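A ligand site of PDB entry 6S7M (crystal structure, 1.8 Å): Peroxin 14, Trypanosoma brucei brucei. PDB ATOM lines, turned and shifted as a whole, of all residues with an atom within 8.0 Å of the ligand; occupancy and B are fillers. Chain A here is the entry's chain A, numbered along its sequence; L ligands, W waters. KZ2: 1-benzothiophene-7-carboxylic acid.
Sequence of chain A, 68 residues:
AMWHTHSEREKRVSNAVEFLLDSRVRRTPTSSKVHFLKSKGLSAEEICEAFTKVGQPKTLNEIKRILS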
ATOM      1  N   VAL A  34      23.278 -11.243   7.145  1.00  0.00           N
ATOM      2  CA  VAL A  34      22.441 -10.090   6.826  1.00  0.00           C
ATOM      3  C   VAL A  34      22.583  -9.010   7.892  1.00  0.00           C
ATOM      4  O   VAL A  34      22.685  -7.816   7.574  1.00  0.00           O
ATOM      5  CB  VAL A  34      20.973 -10.532   6.679  1.00  0.00           C
ATOM      6  CG1 VAL A  34      20.042  -9.313   6.688  1.00  0.00           C
ATOM      7  CG2 VAL A  34      20.814 -11.327   5.414  1.00  0.00           C
ATOM      8  N   LYS A  38      24.019  -5.225   7.256  1.00  0.00           N
ATOM      9  CA  LYS A  38      23.259  -4.046   7.660  1.00  0.00           C
ATOM     10  C   LYS A  38      24.078  -3.146   8.581  1.00  0.00           C
ATOM     11  O   LYS A  38      23.980  -1.914   8.499  1.00  0.00           O
ATOM     12  CB  LYS A  38      21.943  -4.474   8.323  1.00  0.00           C
ATOM     13  CG  LYS A  38      21.035  -3.329   8.772  1.00  0.00           C
ATOM     14  CD  LYS A  38      20.416  -2.578   7.584  1.00  0.00           C
ATOM     15  CE  LYS A  38      19.520  -1.428   8.051  1.00  0.00           C
ATOM     16  NZ  LYS A  38      18.779  -0.799   6.890  1.00  0.00           N
ATOM     17  N   GLY A  41      26.205  -0.699   6.754  1.00  0.00           N
ATOM     18  CA  GLY A  41      25.560   0.348   6.003  1.00  0.00           C
ATOM     19  C   GLY A  41      24.840  -0.086   4.748  1.00  0.00           C
ATOM     20  O   GLY A  41      24.298   0.774   4.048  1.00  0.00           O
ATOM     21  N   LEU A  42      24.806  -1.382   4.432  1.00  0.00           N
ATOM     22  CA  LEU A  42      24.043  -1.832   3.270  1.00  0.00           C
ATOM     23  C   LEU A  42      22.557  -1.798   3.592  1.00  0.00           C
ATOM     24  O   LEU A  42      22.120  -2.179   4.679  1.00  0.00           O
ATOM     25  CB  LEU A  42      24.434  -3.245   2.851  1.00  0.00           C
ATOM     26  CG  LEU A  42      25.695  -3.388   2.007  1.00  0.00           C
ATOM     27  CD1 LEU A  42      26.942  -3.293   2.883  1.00  0.00           C
ATOM     28  CD2 LEU A  42      25.680  -4.704   1.249  1.00  0.00           C
ATOM     29  N   SER A  43      21.783  -1.322   2.634  1.00  0.00           N
ATOM     30  CA  SER A  43      20.340  -1.474   2.700  1.00  0.00           C
ATOM     31  C   SER A  43      19.948  -2.910   2.384  1.00  0.00           C
ATOM     32  O   SER A  43      20.721  -3.688   1.813  1.00  0.00           O
ATOM     33  CB  SER A  43      19.677  -0.555   1.687  1.00  0.00           C
ATOM     34  OG  SER A  43      20.049  -0.969   0.376  1.00  0.00           O
ATOM     35  N   ALA A  44      18.691  -3.247   2.710  1.00  0.00           N
ATOM     36  CA  ALA A  44      18.165  -4.558   2.332  1.00  0.00           C
ATOM     37  C   ALA A  44      18.297  -4.809   0.835  1.00  0.00           C
ATOM     38  O   ALA A  44      18.636  -5.916   0.413  1.00  0.00           O
ATOM     39  CB  ALA A  44      16.695  -4.673   2.738  1.00  0.00           C
ATOM     40  N   GLU A  45      18.046  -3.778   0.025  1.00  0.00           N
ATOM     41  CA  GLU A  45      18.187  -3.926  -1.421  1.00  0.00           C
ATOM     42  C   GLU A  45      19.634  -4.225  -1.813  1.00  0.00           C
ATOM     43  O   GLU A  45      19.883  -5.087  -2.666  1.00  0.00           O
ATOM     44  CB  GLU A  45      17.672  -2.664  -2.117  1.00  0.00           C
ATOM     45  N   GLU A  46      20.601  -3.557  -1.166  1.00  0.00           N
ATOM     46  CA  GLU A  46      21.996  -3.836  -1.487  1.00  0.00           C
ATOM     47  C   GLU A  46      22.418  -5.216  -0.997  1.00  0.00           C
ATOM     48  O   GLU A  46      23.177  -5.921  -1.679  1.00  0.00           O
ATOM     49  CB  GLU A  46      22.905  -2.739  -0.884  1.00  0.00           C
ATOM     50  CG  GLU A  46      22.676  -1.362  -1.511  1.00  0.00           C
ATOM     51  CD  GLU A  46      23.309  -0.215  -0.737  1.00  0.00           C
ATOM     52  OE1 GLU A  46      23.872  -0.461   0.345  1.00  0.00           O
ATOM     53  OE2 GLU A  46      23.233   0.940  -1.209  1.00  0.00           O
ATOM     54  N   ILE A  47      21.918  -5.637   0.164  1.00  0.00           N
ATOM     55  CA  ILE A  47      22.172  -7.000   0.640  1.00  0.00           C
ATOM     56  C   ILE A  47      21.630  -8.007  -0.353  1.00  0.00           C
ATOM     57  O   ILE A  47      22.274  -9.030  -0.644  1.00  0.00           O
ATOM     58  CB  ILE A  47      21.547  -7.198   2.032  1.00  0.00           C
ATOM     59  CG1 ILE A  47      22.228  -6.262   3.029  1.00  0.00           C
ATOM     60  CG2 ILE A  47      21.689  -8.664   2.467  1.00  0.00           C
ATOM     61  CD1 ILE A  47      21.548  -6.217   4.393  1.00  0.00           C
ATOM     62  N   LEU A  60      13.867 -10.079  -1.448  1.00  0.00           N
ATOM     63  CA  LEU A  60      13.869  -8.845  -0.669  1.00  0.00           C
ATOM     64  C   LEU A  60      13.088  -9.017   0.628  1.00  0.00           C
ATOM     65  O   LEU A  60      13.528  -8.566   1.694  1.00  0.00           O
ATOM     66  CB  LEU A  60      13.332  -7.689  -1.510  1.00  0.00           C
ATOM     67  CG  LEU A  60      13.370  -6.315  -0.848  1.00  0.00           C
ATOM     68  CD1 LEU A  60      14.803  -5.973  -0.497  1.00  0.00           C
ATOM     69  CD2 LEU A  60      12.822  -5.294  -1.834  1.00  0.00           C
ATOM     70  N   ASN A  61      11.938  -9.696   0.574  1.00  0.00           N
ATOM     71  CA  ASN A  61      11.143  -9.838   1.795  1.00  0.00           C
ATOM     72  C   ASN A  61      11.872 -10.656   2.855  1.00  0.00           C
ATOM     73  O   ASN A  61      11.820 -10.334   4.047  1.00  0.00           O
ATOM     74  CB  ASN A  61       9.780 -10.441   1.493  1.00  0.00           C
ATOM     75  CG  ASN A  61       8.786  -9.413   1.015  1.00  0.00           C
ATOM     76  OD1 ASN A  61       8.933  -8.219   1.285  1.00  0.00           O
ATOM     77  ND2 ASN A  61       7.758  -9.857   0.297  1.00  0.00           N
ATOM     78  N   ILE A  63      15.011 -10.802   3.364  1.00  0.00           N
ATOM     79  CA  ILE A  63      16.033  -9.950   3.969  1.00  0.00           C
ATOM     80  C   ILE A  63      15.376  -8.936   4.904  1.00  0.00           C
ATOM     81  O   ILE A  63      15.841  -8.716   6.022  1.00  0.00           O
ATOM     82  CB  ILE A  63      16.886  -9.259   2.903  1.00  0.00           C
ATOM     83  CG1 ILE A  63      17.643 -10.285   2.057  1.00  0.00           C
ATOM     84  CG2 ILE A  63      17.848  -8.262   3.553  1.00  0.00           C
ATOM     85  CD1 ILE A  63      18.448 -11.262   2.877  1.00  0.00           C
ATOM     86  N   LYS A  64      14.301  -8.298   4.447  1.00  0.00           N
ATOM     87  CA  LYS A  64      13.614  -7.335   5.296  1.00  0.00           C
ATOM     88  C   LYS A  64      13.073  -8.013   6.543  1.00  0.00           C
ATOM     89  O   LYS A  64      13.106  -7.420   7.632  1.00  0.00           O
ATOM     90  CB  LYS A  64      12.476  -6.663   4.520  1.00  0.00           C
ATOM     91  CG  LYS A  64      12.947  -5.634   3.506  1.00  0.00           C
ATOM     92  CD  LYS A  64      11.753  -5.090   2.727  1.00  0.00           C
ATOM     93  CE  LYS A  64      12.147  -3.974   1.796  1.00  0.00           C
ATOM     94  NZ  LYS A  64      10.929  -3.456   1.133  1.00  0.00           N
ATOM     95  N   ARG A  65      12.579  -9.234   6.413  1.00  0.00           N
ATOM     96  CA  ARG A  65      12.008  -9.908   7.574  1.00  0.00           C
ATOM     97  C   ARG A  65      13.083 -10.200   8.619  1.00  0.00           C
ATOM     98  O   ARG A  65      12.800 -10.127   9.823  1.00  0.00           O
ATOM     99  CB  ARG A  65      11.288 -11.189   7.140  1.00  0.00           C
ATOM    100  CG  ARG A  65       9.955 -10.925   6.462  1.00  0.00           C
ATOM    101  N   ILE A  66      14.311 -10.491   8.189  1.00  0.00           N
ATOM    102  CA  ILE A  66      15.400 -10.678   9.151  1.00  0.00           C
ATOM    103  C   ILE A  66      15.677  -9.377   9.896  1.00  0.00           C
ATOM    104  O   ILE A  66      15.929  -9.383  11.112  1.00  0.00           O
ATOM    105  CB  ILE A  66      16.661 -11.184   8.420  1.00  0.00           C
ATOM    106  CG1 ILE A  66      16.445 -12.592   7.859  1.00  0.00           C
ATOM    107  CG2 ILE A  66      17.870 -11.150   9.365  1.00  0.00           C
ATOM    108  CD1 ILE A  66      17.486 -12.996   6.822  1.00  0.00           C
ATOM    109  N   LEU A  67      15.662  -8.254   9.193  1.00  0.00           N
ATOM    110  CA  LEU A  67      16.083  -6.989   9.781  1.00  0.00           C
ATOM    111  C   LEU A  67      14.982  -6.226  10.520  1.00  0.00           C
ATOM    112  O   LEU A  67      15.305  -5.282  11.250  1.00  0.00           O
ATOM    113  CB  LEU A  67      16.668  -6.084   8.717  1.00  0.00           C
ATOM    114  CG  LEU A  67      17.900  -6.643   7.998  1.00  0.00           C
ATOM    115  CD1 LEU A  67      18.185  -5.768   6.766  1.00  0.00           C
ATOM    116  CD2 LEU A  67      19.095  -6.679   8.924  1.00  0.00           C
ATOM    117  N   SER A  68      13.726  -6.628  10.380  1.00  0.00           N
ATOM    118  CA  SER A  68      12.641  -5.869  10.989  1.00  0.00           C
ATOM    119  C   SER A  68      12.456  -6.205  12.466  1.00  0.00           C
ATOM    120  O   SER A  68      11.741  -5.487  13.177  1.00  0.00           O
ATOM    121  CB  SER A  68      11.347  -6.099  10.227  1.00  0.00           C
ATOM    122  OG  SER A  68      11.472  -5.643   8.888  1.00  0.00           O
ATOM    123  OXT SER A  68      13.002  -7.182  12.986  1.00  0.00           O
HETATM  124  C7  KZ2 L   1      13.847  -3.839   6.639  1.00  0.00           C
HETATM  125  C6  KZ2 L   1      12.602  -3.411   6.211  1.00  0.00           C
HETATM  126  C8  KZ2 L   1      15.010  -3.326   6.101  1.00  0.00           C
HETATM  127  C3  KZ2 L   1      11.657  -0.929   3.649  1.00  0.00           C
HETATM  128  C1  KZ2 L   1      14.934  -2.345   5.109  1.00  0.00           C
HETATM  129  C2  KZ2 L   1      13.677  -1.912   4.676  1.00  0.00           C
HETATM  130  C5  KZ2 L   1      12.481  -2.432   5.204  1.00  0.00           C
HETATM  131  O1  KZ2 L   1      17.295  -2.197   5.065  1.00  0.00           O
HETATM  132  C   KZ2 L   1      16.233  -1.792   4.544  1.00  0.00           C
HETATM  133  O   KZ2 L   1      16.186  -0.976   3.583  1.00  0.00           O
HETATM  134  C4  KZ2 L   1      11.326  -1.843   4.583  1.00  0.00           C
HETATM  135  S   KZ2 L   1      13.351  -0.720   3.466  1.00  0.00           S
HETATM  136  O   HOH W   1      16.249  -1.505   0.735  1.00  0.00           O
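Ser 43 touches the ligand (C to O1, 3.8 Å).
CG of Lys 64 touches C6 of the ligand, 3.5 Å away.
Ser 68 touches the ligand (OG to C6, 3.7 Å).
Hydrophobic or aromatic side chains that line the ligand: Ala 44.
Of the 17 residues printed, 5 come within 4 Å of the ligand.
The nearest printed residue that does not touch the ligand is Leu 67 (4.1 Å).
An oxygen (O1) of the ligand sits at hydrogen-bond distance from the backbone NH (N) of Ala 44 (2.9 Å).
The side-chain amino group (NZ) of Lys 38 is in salt-bridge range of an oxygen (O1) of the ligand (2.7 Å).
O of Lys 64 lies within hydrogen-bond range of OG of Ser 68 (2.7 Å).
The side-chain hydroxyl of Ser 43 sits close to the backbone NH of Glu 45 (3.5 Å).
The side-chain hydroxyl (OG) of Ser 43 lies within hydrogen-bond range of the backbone NH (N) of Glu 46 (3.1 Å).
Water W1 lies within hydrogen-bond range of an oxygen (O) of the ligand (2.9 Å) and the backbone NH (N) of Glu 45 (3.0 Å).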
